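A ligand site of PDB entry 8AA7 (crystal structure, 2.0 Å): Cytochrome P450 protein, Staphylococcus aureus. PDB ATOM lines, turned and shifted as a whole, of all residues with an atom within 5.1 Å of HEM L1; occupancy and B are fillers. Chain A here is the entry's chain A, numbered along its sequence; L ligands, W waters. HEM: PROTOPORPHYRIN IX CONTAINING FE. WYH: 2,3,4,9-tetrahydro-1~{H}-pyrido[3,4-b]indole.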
ATOM      1  N   LEU A  52     -13.817  20.989  21.826  1.00  0.00           N
ATOM      2  CA  LEU A  52     -14.612  19.922  21.202  1.00  0.00           C
ATOM      3  C   LEU A  52     -15.509  20.461  20.091  1.00  0.00           C
ATOM      4  O   LEU A  52     -15.848  19.717  19.156  1.00  0.00           O
ATOM      5  CB  LEU A  52     -15.445  19.184  22.257  1.00  0.00           C
ATOM      6  CG  LEU A  52     -14.622  18.470  23.367  1.00  0.00           C
ATOM      7  CD1 LEU A  52     -15.480  17.948  24.528  1.00  0.00           C
ATOM      8  CD2 LEU A  52     -13.841  17.282  22.770  1.00  0.00           C
ATOM      9  N   THR A  60      -8.849  14.877  15.525  1.00  0.00           N
ATOM     10  CA  THR A  60      -8.818  13.582  16.182  1.00  0.00           C
ATOM     11  C   THR A  60      -7.683  12.694  15.678  1.00  0.00           C
ATOM     12  O   THR A  60      -7.709  11.484  15.925  1.00  0.00           O
ATOM     13  CB  THR A  60     -10.152  12.872  15.996  1.00  0.00           C
ATOM     14  OG1 THR A  60     -10.545  12.961  14.624  1.00  0.00           O
ATOM     15  CG2 THR A  60     -11.229  13.511  16.847  1.00  0.00           C
ATOM     16  N   LEU A  63      -5.971   9.877  17.841  1.00  0.00           N
ATOM     17  CA  LEU A  63      -6.524   8.540  17.991  1.00  0.00           C
ATOM     18  C   LEU A  63      -5.959   7.543  16.990  1.00  0.00           C
ATOM     19  O   LEU A  63      -6.325   6.359  17.041  1.00  0.00           O
ATOM     20  CB  LEU A  63      -8.055   8.587  17.880  1.00  0.00           C
ATOM     21  CG  LEU A  63      -8.798   9.100  19.129  1.00  0.00           C
ATOM     22  CD1 LEU A  63      -9.242  10.545  18.952  1.00  0.00           C
ATOM     23  CD2 LEU A  63      -9.987   8.198  19.452  1.00  0.00           C
ATOM     24  N   LEU A  76     -14.125   5.294  13.757  1.00  0.00           N
ATOM     25  CA  LEU A  76     -15.032   6.373  13.389  1.00  0.00           C
ATOM     26  C   LEU A  76     -14.467   7.741  13.748  1.00  0.00           C
ATOM     27  O   LEU A  76     -14.723   8.729  13.050  1.00  0.00           O
ATOM     28  CB  LEU A  76     -16.387   6.153  14.064  1.00  0.00           C
ATOM     29  CG  LEU A  76     -17.479   7.203  13.769  1.00  0.00           C
ATOM     30  CD1 LEU A  76     -17.985   7.081  12.323  1.00  0.00           C
ATOM     31  CD2 LEU A  76     -18.644   7.068  14.760  1.00  0.00           C
ATOM     32  N   ALA A  77     -13.681   7.830  14.833  1.00  0.00           N
ATOM     33  CA  ALA A  77     -13.128   9.102  15.268  1.00  0.00           C
ATOM     34  C   ALA A  77     -12.206   9.704  14.212  1.00  0.00           C
ATOM     35  O   ALA A  77     -12.164  10.925  14.042  1.00  0.00           O
ATOM     36  CB  ALA A  77     -12.388   8.946  16.588  1.00  0.00           C
ATOM     37  N   HIS A  84     -17.734  10.308   7.791  1.00  0.00           N
ATOM     38  CA  HIS A  84     -17.993  10.207   9.221  1.00  0.00           C
ATOM     39  C   HIS A  84     -19.488  10.311   9.495  1.00  0.00           C
ATOM     40  O   HIS A  84     -20.031   9.567  10.322  1.00  0.00           O
ATOM     41  CB  HIS A  84     -17.246  11.309   9.967  1.00  0.00           C
ATOM     42  CG  HIS A  84     -17.700  11.495  11.378  1.00  0.00           C
ATOM     43  ND1 HIS A  84     -18.683  12.395  11.735  1.00  0.00           N
ATOM     44  CD2 HIS A  84     -17.350  10.856  12.529  1.00  0.00           C
ATOM     45  CE1 HIS A  84     -18.901  12.326  13.039  1.00  0.00           C
ATOM     46  NE2 HIS A  84     -18.089  11.404  13.542  1.00  0.00           N
ATOM     47  N   LYS A  88     -21.378   7.113  10.965  1.00  0.00           N
ATOM     48  CA  LYS A  88     -21.968   7.337  12.279  1.00  0.00           C
ATOM     49  C   LYS A  88     -23.475   7.064  12.244  1.00  0.00           C
ATOM     50  O   LYS A  88     -24.026   6.456  13.164  1.00  0.00           O
ATOM     51  CB  LYS A  88     -21.666   8.768  12.747  1.00  0.00           C
ATOM     52  CG  LYS A  88     -22.177   9.098  14.142  1.00  0.00           C
ATOM     53  CD  LYS A  88     -21.652  10.427  14.654  1.00  0.00           C
ATOM     54  CE  LYS A  88     -21.944  10.667  16.115  1.00  0.00           C
ATOM     55  NZ  LYS A  88     -21.127  11.859  16.660  1.00  0.00           N
ATOM     56  N   ILE A  91     -24.115   3.418  12.323  1.00  0.00           N
ATOM     57  CA  ILE A  91     -23.947   2.808  13.636  1.00  0.00           C
ATOM     58  C   ILE A  91     -25.144   3.130  14.524  1.00  0.00           C
ATOM     59  O   ILE A  91     -25.625   2.275  15.265  1.00  0.00           O
ATOM     60  CB  ILE A  91     -22.614   3.253  14.273  1.00  0.00           C
ATOM     61  CG1 ILE A  91     -21.442   2.712  13.454  1.00  0.00           C
ATOM     62  CG2 ILE A  91     -22.487   2.783  15.718  1.00  0.00           C
ATOM     63  CD1 ILE A  91     -20.117   3.211  13.905  1.00  0.00           C
ATOM     64  N   MET A  95     -28.851   0.871  17.016  1.00  0.00           N
ATOM     65  CA  MET A  95     -29.312   1.045  18.386  1.00  0.00           C
ATOM     66  C   MET A  95     -30.528   1.979  18.418  1.00  0.00           C
ATOM     67  O   MET A  95     -30.846   2.548  19.461  1.00  0.00           O
ATOM     68  CB  MET A  95     -28.171   1.561  19.269  1.00  0.00           C
ATOM     69  CG  MET A  95     -27.530   2.901  18.828  1.00  0.00           C
ATOM     70  SD  MET A  95     -25.908   3.134  19.615  1.00  0.00           S
ATOM     71  CE  MET A  95     -24.805   2.180  18.599  1.00  0.00           C
ATOM     72  N   LEU A 142     -25.832  -6.150  20.893  1.00  0.00           N
ATOM     73  CA  LEU A 142     -25.931  -5.030  19.957  1.00  0.00           C
ATOM     74  C   LEU A 142     -25.246  -5.370  18.641  1.00  0.00           C
ATOM     75  O   LEU A 142     -25.818  -5.159  17.562  1.00  0.00           O
ATOM     76  CB  LEU A 142     -25.310  -3.768  20.586  1.00  0.00           C
ATOM     77  CG  LEU A 142     -25.132  -2.538  19.667  1.00  0.00           C
ATOM     78  CD1 LEU A 142     -26.474  -2.062  19.189  1.00  0.00           C
ATOM     79  CD2 LEU A 142     -24.420  -1.476  20.439  1.00  0.00           C
ATOM     80  N   ASN A 228     -14.543  -1.023  17.683  1.00  0.00           N
ATOM     81  CA  ASN A 228     -14.806   0.286  18.250  1.00  0.00           C
ATOM     82  C   ASN A 228     -16.082   0.272  19.081  1.00  0.00           C
ATOM     83  O   ASN A 228     -16.105   0.770  20.218  1.00  0.00           O
ATOM     84  CB  ASN A 228     -14.897   1.350  17.153  1.00  0.00           C
ATOM     85  CG  ASN A 228     -15.048   2.770  17.721  1.00  0.00           C
ATOM     86  OD1 ASN A 228     -14.911   2.977  18.930  1.00  0.00           O
ATOM     87  ND2 ASN A 228     -15.321   3.741  16.855  1.00  0.00           N
ATOM     88  N   VAL A 229     -17.152  -0.318  18.536  1.00  0.00           N
ATOM     89  CA  VAL A 229     -18.434  -0.371  19.240  1.00  0.00           C
ATOM     90  C   VAL A 229     -18.327  -1.261  20.478  1.00  0.00           C
ATOM     91  O   VAL A 229     -18.834  -0.923  21.553  1.00  0.00           O
ATOM     92  CB  VAL A 229     -19.555  -0.814  18.281  1.00  0.00           C
ATOM     93  CG1 VAL A 229     -20.817  -1.282  19.038  1.00  0.00           C
ATOM     94  CG2 VAL A 229     -19.895   0.331  17.314  1.00  0.00           C
ATOM     95  N   ALA A 232     -16.197   0.703  22.925  1.00  0.00           N
ATOM     96  CA  ALA A 232     -16.885   1.903  23.381  1.00  0.00           C
ATOM     97  C   ALA A 232     -18.097   1.584  24.248  1.00  0.00           C
ATOM     98  O   ALA A 232     -18.344   2.263  25.245  1.00  0.00           O
ATOM     99  CB  ALA A 232     -17.307   2.741  22.170  1.00  0.00           C
ATOM    100  N   ALA A 233     -18.876   0.561  23.877  1.00  0.00           N
ATOM    101  CA  ALA A 233     -20.110   0.271  24.595  1.00  0.00           C
ATOM    102  C   ALA A 233     -19.886  -0.462  25.916  1.00  0.00           C
ATOM    103  O   ALA A 233     -20.696  -0.309  26.830  1.00  0.00           O
ATOM    104  CB  ALA A 233     -21.072  -0.536  23.717  1.00  0.00           C
ATOM    105  N   PRO A 236     -17.849   1.965  29.735  1.00  0.00           N
ATOM    106  CA  PRO A 236     -18.467   2.932  30.663  1.00  0.00           C
ATOM    107  C   PRO A 236     -19.659   2.400  31.446  1.00  0.00           C
ATOM    108  O   PRO A 236     -20.109   3.111  32.373  1.00  0.00           O
ATOM    109  CB  PRO A 236     -18.931   4.079  29.741  1.00  0.00           C
ATOM    110  CG  PRO A 236     -18.348   3.758  28.361  1.00  0.00           C
ATOM    111  CD  PRO A 236     -18.157   2.267  28.333  1.00  0.00           C
ATOM    112  N   THR A 240     -20.698   3.342  35.333  1.00  0.00           N
ATOM    113  CA  THR A 240     -21.785   4.290  35.560  1.00  0.00           C
ATOM    114  C   THR A 240     -22.858   3.672  36.429  1.00  0.00           C
ATOM    115  O   THR A 240     -23.426   4.353  37.295  1.00  0.00           O
ATOM    116  CB  THR A 240     -22.390   4.758  34.230  1.00  0.00           C
ATOM    117  OG1 THR A 240     -21.382   5.392  33.437  1.00  0.00           O
ATOM    118  CG2 THR A 240     -23.542   5.737  34.447  1.00  0.00           C
ATOM    119  N   LEU A 273     -23.406  10.859  35.549  1.00  0.00           N
ATOM    120  CA  LEU A 273     -22.446  11.003  34.468  1.00  0.00           C
ATOM    121  C   LEU A 273     -21.684  12.311  34.594  1.00  0.00           C
ATOM    122  O   LEU A 273     -20.481  12.358  34.335  1.00  0.00           O
ATOM    123  CB  LEU A 273     -23.146  10.931  33.112  1.00  0.00           C
ATOM    124  CG  LEU A 273     -23.621   9.522  32.749  1.00  0.00           C
ATOM    125  CD1 LEU A 273     -24.591   9.522  31.588  1.00  0.00           C
ATOM    126  CD2 LEU A 273     -22.392   8.629  32.472  1.00  0.00           C
ATOM    127  N   PRO A 278     -17.409   8.776  33.672  1.00  0.00           N
ATOM    128  CA  PRO A 278     -16.654   7.521  33.505  1.00  0.00           C
ATOM    129  C   PRO A 278     -15.596   7.601  32.418  1.00  0.00           C
ATOM    130  O   PRO A 278     -14.580   6.911  32.526  1.00  0.00           O
ATOM    131  CB  PRO A 278     -17.722   6.479  33.157  1.00  0.00           C
ATOM    132  CG  PRO A 278     -18.921   7.275  32.633  1.00  0.00           C
ATOM    133  CD  PRO A 278     -18.753   8.716  33.054  1.00  0.00           C
ATOM    134  N   VAL A 279     -15.807   8.368  31.351  1.00  0.00           N
ATOM    135  CA  VAL A 279     -14.756   8.714  30.410  1.00  0.00           C
ATOM    136  C   VAL A 279     -14.176  10.062  30.853  1.00  0.00           C
ATOM    137  O   VAL A 279     -14.836  11.098  30.746  1.00  0.00           O
ATOM    138  CB  VAL A 279     -15.290   8.771  28.972  1.00  0.00           C
ATOM    139  CG1 VAL A 279     -14.179   9.075  28.014  1.00  0.00           C
ATOM    140  CG2 VAL A 279     -15.974   7.453  28.607  1.00  0.00           C
ATOM    141  N   ILE A 282     -10.454  13.253  26.928  1.00  0.00           N
ATOM    142  CA  ILE A 282     -10.624  13.240  25.479  1.00  0.00           C
ATOM    143  C   ILE A 282      -9.447  13.967  24.846  1.00  0.00           C
ATOM    144  O   ILE A 282      -9.316  15.191  25.003  1.00  0.00           O
ATOM    145  CB  ILE A 282     -11.945  13.895  25.077  1.00  0.00           C
ATOM    146  CG1 ILE A 282     -13.140  13.185  25.704  1.00  0.00           C
ATOM    147  CG2 ILE A 282     -12.099  13.904  23.541  1.00  0.00           C
ATOM    148  CD1 ILE A 282     -14.449  13.907  25.263  1.00  0.00           C
ATOM    149  N   PRO A 283      -8.599  13.274  24.093  1.00  0.00           N
ATOM    150  CA  PRO A 283      -7.480  13.944  23.431  1.00  0.00           C
ATOM    151  C   PRO A 283      -7.856  14.502  22.059  1.00  0.00           C
ATOM    152  O   PRO A 283      -8.758  14.016  21.376  1.00  0.00           O
ATOM    153  CB  PRO A 283      -6.447  12.820  23.301  1.00  0.00           C
ATOM    154  CG  PRO A 283      -7.269  11.575  23.184  1.00  0.00           C
ATOM    155  CD  PRO A 283      -8.566  11.812  23.885  1.00  0.00           C
ATOM    156  N   ARG A 284      -7.101  15.546  21.693  1.00  0.00           N
ATOM    157  CA  ARG A 284      -7.177  16.223  20.420  1.00  0.00           C
ATOM    158  C   ARG A 284      -5.768  16.679  20.057  1.00  0.00           C
ATOM    159  O   ARG A 284      -4.913  16.856  20.928  1.00  0.00           O
ATOM    160  CB  ARG A 284      -8.137  17.430  20.435  1.00  0.00           C
ATOM    161  CG  ARG A 284      -9.595  17.091  20.583  1.00  0.00           C
ATOM    162  CD  ARG A 284     -10.099  16.330  19.370  1.00  0.00           C
ATOM    163  NE  ARG A 284     -11.554  16.181  19.375  1.00  0.00           N
ATOM    164  CZ  ARG A 284     -12.204  15.106  19.799  1.00  0.00           C
ATOM    165  NH1 ARG A 284     -11.572  14.052  20.278  1.00  0.00           N
ATOM    166  NH2 ARG A 284     -13.540  15.081  19.725  1.00  0.00           N
ATOM    167  N   LEU A 342     -20.590  17.383  29.654  1.00  0.00           N
ATOM    168  CA  LEU A 342     -19.754  16.965  28.542  1.00  0.00           C
ATOM    169  C   LEU A 342     -19.395  15.480  28.650  1.00  0.00           C
ATOM    170  O   LEU A 342     -18.431  15.021  28.021  1.00  0.00           O
ATOM    171  CB  LEU A 342     -18.493  17.839  28.464  1.00  0.00           C
ATOM    172  CG  LEU A 342     -18.752  19.339  28.298  1.00  0.00           C
ATOM    173  CD1 LEU A 342     -17.552  20.191  28.673  1.00  0.00           C
ATOM    174  CD2 LEU A 342     -19.144  19.594  26.883  1.00  0.00           C
ATOM    175  N   SER A 343     -20.180  14.717  29.418  1.00  0.00           N
ATOM    176  CA  SER A 343     -19.842  13.322  29.666  1.00  0.00           C
ATOM    177  C   SER A 343     -19.924  12.470  28.403  1.00  0.00           C
ATOM    178  O   SER A 343     -19.289  11.419  28.321  1.00  0.00           O
ATOM    179  CB  SER A 343     -20.760  12.751  30.741  1.00  0.00           C
ATOM    180  OG  SER A 343     -22.063  12.591  30.245  1.00  0.00           O
ATOM    181  N   PHE A 344     -20.719  12.910  27.423  1.00  0.00           N
ATOM    182  CA  PHE A 344     -20.803  12.308  26.100  1.00  0.00           C
ATOM    183  C   PHE A 344     -20.054  13.106  25.049  1.00  0.00           C
ATOM    184  O   PHE A 344     -20.228  12.859  23.852  1.00  0.00           O
ATOM    185  CB  PHE A 344     -22.256  12.181  25.671  1.00  0.00           C
ATOM    186  CG  PHE A 344     -23.032  11.173  26.463  1.00  0.00           C
ATOM    187  CD1 PHE A 344     -22.708   9.815  26.404  1.00  0.00           C
ATOM    188  CD2 PHE A 344     -24.128  11.570  27.233  1.00  0.00           C
ATOM    189  CE1 PHE A 344     -23.429   8.849  27.134  1.00  0.00           C
ATOM    190  CE2 PHE A 344     -24.908  10.589  27.932  1.00  0.00           C
ATOM    191  CZ  PHE A 344     -24.525   9.246  27.904  1.00  0.00           C
ATOM    192  N   GLY A 345     -19.214  14.059  25.468  1.00  0.00           N
ATOM    193  CA  GLY A 345     -18.570  14.986  24.554  1.00  0.00           C
ATOM    194  C   GLY A 345     -19.581  15.970  24.001  1.00  0.00           C
ATOM    195  O   GLY A 345     -20.694  16.165  24.518  1.00  0.00           O
ATOM    196  N   VAL A 348     -18.854  17.442  16.697  1.00  0.00           N
ATOM    197  CA  VAL A 348     -18.963  16.453  15.619  1.00  0.00           C
ATOM    198  C   VAL A 348     -18.843  15.025  16.155  1.00  0.00           C
ATOM    199  O   VAL A 348     -19.478  14.080  15.634  1.00  0.00           O
ATOM    200  CB  VAL A 348     -17.887  16.740  14.558  1.00  0.00           C
ATOM    201  CG1 VAL A 348     -17.752  15.542  13.606  1.00  0.00           C
ATOM    202  CG2 VAL A 348     -18.161  18.023  13.771  1.00  0.00           C
ATOM    203  N   HIS A 349     -17.993  14.811  17.156  1.00  0.00           N
ATOM    204  CA  HIS A 349     -17.679  13.447  17.574  1.00  0.00           C
ATOM    205  C   HIS A 349     -18.407  13.069  18.847  1.00  0.00           C
ATOM    206  O   HIS A 349     -17.998  12.136  19.530  1.00  0.00           O
ATOM    207  CB  HIS A 349     -16.176  13.285  17.728  1.00  0.00           C
ATOM    208  CG  HIS A 349     -15.432  13.296  16.421  1.00  0.00           C
ATOM    209  ND1 HIS A 349     -15.549  12.278  15.494  1.00  0.00           N
ATOM    210  CD2 HIS A 349     -14.579  14.199  15.876  1.00  0.00           C
ATOM    211  CE1 HIS A 349     -14.785  12.543  14.451  1.00  0.00           C
ATOM    212  NE2 HIS A 349     -14.202  13.704  14.654  1.00  0.00           N
ATOM    213  N   THR A 350     -19.475  13.786  19.182  1.00  0.00           N
ATOM    214  CA  THR A 350     -20.282  13.459  20.345  1.00  0.00           C
ATOM    215  C   THR A 350     -20.738  12.010  20.265  1.00  0.00           C
ATOM    216  O   THR A 350     -20.991  11.460  19.187  1.00  0.00           O
ATOM    217  CB  THR A 350     -21.487  14.393  20.425  1.00  0.00           C
ATOM    218  OG1 THR A 350     -22.090  14.314  21.725  1.00  0.00           O
ATOM    219  CG2 THR A 350     -22.543  14.020  19.416  1.00  0.00           C
ATOM    220  N   CYS A 351     -20.875  11.387  21.439  1.00  0.00           N
ATOM    221  CA  CYS A 351     -21.101   9.947  21.519  1.00  0.00           C
ATOM    222  C   CYS A 351     -22.345   9.504  20.739  1.00  0.00           C
ATOM    223  O   CYS A 351     -23.461   9.907  21.049  1.00  0.00           O
ATOM    224  CB  CYS A 351     -21.245   9.535  22.974  1.00  0.00           C
ATOM    225  SG  CYS A 351     -21.539   7.731  23.111  1.00  0.00           S
ATOM    226  N   VAL A 352     -22.139   8.638  19.746  1.00  0.00           N
ATOM    227  CA  VAL A 352     -23.268   8.086  19.005  1.00  0.00           C
ATOM    228  C   VAL A 352     -24.149   7.215  19.892  1.00  0.00           C
ATOM    229  O   VAL A 352     -25.342   7.054  19.608  1.00  0.00           O
ATOM    230  CB  VAL A 352     -22.763   7.305  17.786  1.00  0.00           C
ATOM    231  CG1 VAL A 352     -22.055   6.022  18.206  1.00  0.00           C
ATOM    232  CG2 VAL A 352     -23.916   7.061  16.800  1.00  0.00           C
ATOM    233  N   GLY A 353     -23.603   6.663  20.960  1.00  0.00           N
ATOM    234  CA  GLY A 353     -24.267   5.765  21.873  1.00  0.00           C
ATOM    235  C   GLY A 353     -25.015   6.440  23.009  1.00  0.00           C
ATOM    236  O   GLY A 353     -25.559   5.730  23.863  1.00  0.00           O
ATOM    237  N   PHE A 356     -28.904   5.556  23.433  1.00  0.00           N
ATOM    238  CA  PHE A 356     -28.998   4.145  23.800  1.00  0.00           C
ATOM    239  C   PHE A 356     -28.515   3.914  25.228  1.00  0.00           C
ATOM    240  O   PHE A 356     -29.174   3.193  25.991  1.00  0.00           O
ATOM    241  CB  PHE A 356     -28.192   3.281  22.817  1.00  0.00           C
ATOM    242  CG  PHE A 356     -28.032   1.854  23.264  1.00  0.00           C
ATOM    243  CD1 PHE A 356     -29.123   1.018  23.349  1.00  0.00           C
ATOM    244  CD2 PHE A 356     -26.798   1.350  23.595  1.00  0.00           C
ATOM    245  CE1 PHE A 356     -28.974  -0.302  23.763  1.00  0.00           C
ATOM    246  CE2 PHE A 356     -26.648   0.030  24.024  1.00  0.00           C
ATOM    247  CZ  PHE A 356     -27.743  -0.793  24.102  1.00  0.00           C
ATOM    248  N   SER A 357     -27.340   4.476  25.574  1.00  0.00           N
ATOM    249  CA  SER A 357     -26.785   4.342  26.921  1.00  0.00           C
ATOM    250  C   SER A 357     -27.779   4.767  27.980  1.00  0.00           C
ATOM    251  O   SER A 357     -27.974   4.067  28.984  1.00  0.00           O
ATOM    252  CB  SER A 357     -25.505   5.184  27.070  1.00  0.00           C
ATOM    253  OG  SER A 357     -24.449   4.592  26.347  1.00  0.00           O
ATOM    254  N   LEU A 361     -29.288   2.133  30.589  1.00  0.00           N
ATOM    255  CA  LEU A 361     -29.016   2.300  32.016  1.00  0.00           C
ATOM    256  C   LEU A 361     -30.302   2.529  32.808  1.00  0.00           C
ATOM    257  O   LEU A 361     -30.387   2.087  33.949  1.00  0.00           O
ATOM    258  CB  LEU A 361     -28.079   3.483  32.248  1.00  0.00           C
ATOM    259  CG  LEU A 361     -26.624   3.295  31.795  1.00  0.00           C
ATOM    260  CD1 LEU A 361     -25.901   4.639  31.809  1.00  0.00           C
ATOM    261  CD2 LEU A 361     -26.000   2.273  32.700  1.00  0.00           C
HETATM  262  CHA HEM L   1     -17.732   8.913  21.552  1.00  0.00           C
HETATM  263  CHB HEM L   1     -18.734   8.782  26.306  1.00  0.00           C
HETATM  264  CHC HEM L   1     -21.466   4.833  25.545  1.00  0.00           C
HETATM  265  CHD HEM L   1     -19.844   4.613  20.993  1.00  0.00           C
HETATM  266  C1A HEM L   1     -17.774   9.272  22.881  1.00  0.00           C
HETATM  267  C2A HEM L   1     -17.204  10.454  23.481  1.00  0.00           C
HETATM  268  C3A HEM L   1     -17.469  10.401  24.796  1.00  0.00           C
HETATM  269  C4A HEM L   1     -18.227   9.205  25.091  1.00  0.00           C
HETATM  270  CMA HEM L   1     -17.109  11.372  25.912  1.00  0.00           C
HETATM  271  CAA HEM L   1     -16.456  11.521  22.646  1.00  0.00           C
HETATM  272  CBA HEM L   1     -15.068  11.024  22.298  1.00  0.00           C
HETATM  273  CGA HEM L   1     -14.342  12.102  21.521  1.00  0.00           C
HETATM  274  O1A HEM L   1     -14.868  13.209  21.244  1.00  0.00           O
HETATM  275  O2A HEM L   1     -13.196  11.852  21.117  1.00  0.00           O
HETATM  276  C1B HEM L   1     -19.603   7.722  26.490  1.00  0.00           C
HETATM  277  C2B HEM L   1     -20.270   7.396  27.741  1.00  0.00           C
HETATM  278  C3B HEM L   1     -21.005   6.275  27.534  1.00  0.00           C
HETATM  279  C4B HEM L   1     -20.836   5.880  26.147  1.00  0.00           C
HETATM  280  CMB HEM L   1     -20.079   8.184  29.062  1.00  0.00           C
HETATM  281  CAB HEM L   1     -21.927   5.530  28.518  1.00  0.00           C
HETATM  282  CBB HEM L   1     -22.196   5.968  29.741  1.00  0.00           C
HETATM  283  C1C HEM L   1     -21.308   4.436  24.230  1.00  0.00           C
HETATM  284  C2C HEM L   1     -22.003   3.343  23.550  1.00  0.00           C
HETATM  285  C3C HEM L   1     -21.545   3.272  22.290  1.00  0.00           C
HETATM  286  C4C HEM L   1     -20.550   4.324  22.132  1.00  0.00           C
HETATM  287  CMC HEM L   1     -23.042   2.494  24.299  1.00  0.00           C
HETATM  288  CAC HEM L   1     -21.916   2.343  21.123  1.00  0.00           C
HETATM  289  CBC HEM L   1     -22.865   1.411  21.251  1.00  0.00           C
HETATM  290  C1D HEM L   1     -19.166   5.785  20.733  1.00  0.00           C
HETATM  291  C2D HEM L   1     -18.583   6.178  19.457  1.00  0.00           C
HETATM  292  C3D HEM L   1     -18.018   7.362  19.597  1.00  0.00           C
HETATM  293  C4D HEM L   1     -18.196   7.750  20.992  1.00  0.00           C
HETATM  294  CMD HEM L   1     -18.624   5.392  18.125  1.00  0.00           C
HETATM  295  CAD HEM L   1     -17.309   8.147  18.464  1.00  0.00           C
HETATM  296  CBD HEM L   1     -18.303   9.215  17.977  1.00  0.00           C
HETATM  297  CGD HEM L   1     -17.735   9.967  16.779  1.00  0.00           C
HETATM  298  O1D HEM L   1     -16.490   9.937  16.528  1.00  0.00           O
HETATM  299  O2D HEM L   1     -18.550  10.611  16.061  1.00  0.00           O
HETATM  300  NA  HEM L   1     -18.377   8.560  23.889  1.00  0.00           N
HETATM  301  NB  HEM L   1     -19.998   6.794  25.531  1.00  0.00           N
HETATM  302  NC  HEM L   1     -20.441   4.983  23.323  1.00  0.00           N
HETATM  303  ND  HEM L   1     -18.890   6.762  21.685  1.00  0.00           N
HETATM  304 FE   HEM L   1     -19.437   6.830  23.556  1.00  0.00          FE
HETATM  305  C1  WYH L   2     -10.809   4.752  25.706  1.00  0.00           C
HETATM  306  C10 WYH L   2     -17.394   5.397  25.341  1.00  0.00           C
HETATM  307  C11 WYH L   2     -16.220   4.527  25.736  1.00  0.00           C
HETATM  308  C2  WYH L   2     -11.574   3.854  26.443  1.00  0.00           C
HETATM  309  C3  WYH L   2     -12.946   3.874  26.391  1.00  0.00           C
HETATM  310  C4  WYH L   2     -13.572   4.807  25.569  1.00  0.00           C
HETATM  311  C5  WYH L   2     -14.929   5.120  25.255  1.00  0.00           C
HETATM  312  C6  WYH L   2     -14.930   6.147  24.366  1.00  0.00           C
HETATM  313  C7  WYH L   2     -12.781   5.717  24.822  1.00  0.00           C
HETATM  314  C8  WYH L   2     -11.389   5.691  24.879  1.00  0.00           C
HETATM  315  C9  WYH L   2     -16.158   6.780  23.794  1.00  0.00           C
HETATM  316  N1  WYH L   2     -13.629   6.530  24.100  1.00  0.00           N
HETATM  317  N2  WYH L   2     -17.292   5.869  23.950  1.00  0.00           N
HETATM  318  O   HOH W   1     -16.906  15.147  21.608  1.00  0.00           O
HETATM  319  O   HOH W   2     -23.952   2.229  27.554  1.00  0.00           O
HETATM  320  O   HOH W   3     -11.673  10.014  22.023  1.00  0.00           O
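FE of HEM L1 is bound by SG of Cys 351, at 2.3 Å.
A ring nitrogen (NE2) of His 84 sits at hydrogen-bond distance from an oxygen (O2D) of HEM L1 (2.7 Å).
An oxygen (O1D) of HEM L1 lies within hydrogen-bond range of a ring nitrogen (ND1) of His 349 (2.7 Å).
NH2 of Arg 284 is in salt-bridge range of O1A of HEM L1, 2.8 Å away.
The side-chain amino group of Lys 88 is in salt-bridge range of an oxygen (O2D) of HEM L1.
A nitrogen (N2) of WYH L2 binds an iron atom (FE) of HEM L1 (2.4 Å).
The backbone carbonyl oxygen (O) of Phe 344 sits at hydrogen-bond distance from the backbone NH (N) of Cys 351 (2.9 Å).
The side-chain sulfur (SG) of Cys 351 lies close to the backbone NH (N) of Gly 353 (3.2 Å).
A ring nitrogen (NE2) of His 84 sits at hydrogen-bond distance from a ring nitrogen (ND1) of His 349, 3.3 Å away.
O of Thr 350 is in hydrogen-bond range of NZ of Lys 88 (2.6 Å).
The side-chain hydroxyl (OG) of Ser 357 is in hydrogen-bond range of the backbone carbonyl oxygen (O) of Gly 353 (2.9 Å).
The side-chain hydroxyl of Thr 350 is in hydrogen-bond range of the backbone carbonyl oxygen of Phe 344, 3.2 Å away.
O of Pro 236 lies within hydrogen-bond range of OG1 of Thr 240, at 2.8 Å.
OG1 of Thr 60 is in hydrogen-bond range of O of Ala 77, at 2.7 Å.
Leu 76 touches HEM L1.
Ala 77 touches HEM L1 (CA to O1D, 3.7 Å).
Met 95 touches HEM L1.
CD2 of Leu 142 touches CBC of HEM L1, at 3.4 Å.
Asn 228 touches HEM L1 (ND2 to CMD, 3.9 Å).
Ala 232 touches HEM L1 (CB to CHD, 3.4 Å).
CB of Ala 233 touches CBC of HEM L1 (3.6 Å).
CB of Pro 236 touches CAB of HEM L1 (3.5 Å).
Thr 240 touches HEM L1.
Leu 273 touches HEM L1.
CG of Pro 278 touches CMB of HEM L1 (3.9 Å).
CG2 of Val 279 touches CHB of HEM L1 (3.8 Å).
Ile 282 touches HEM L1 (CG2 to O2A, 3.4 Å).
O of Ser 343 touches CMA of HEM L1, at 3.2 Å.
Phe 344 touches HEM L1 (C to CMA, 3.5 Å).
Gly 345 touches HEM L1 (N to CMA, 3.4 Å).
Val 348 touches HEM L1 (O to O2D, 3.6 Å).
Thr 350 touches HEM L1 (O to CBD, 3.7 Å).
CG1 of Val 352 touches CMD of HEM L1 (3.5 Å).
Gly 353 touches HEM L1 (CA to C3C, 3.7 Å).
Phe 356 touches HEM L1.
Ser 357 touches HEM L1.
Hydrophobic or aromatic side chains that line HEM L1: Leu 76, His 84, Met 95, Leu 142, Ala 232, Ala 233, Pro 236, Leu 273, Pro 278, Val 279, Ile 282, Phe 344, His 349, Val 352 and Phe 356.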
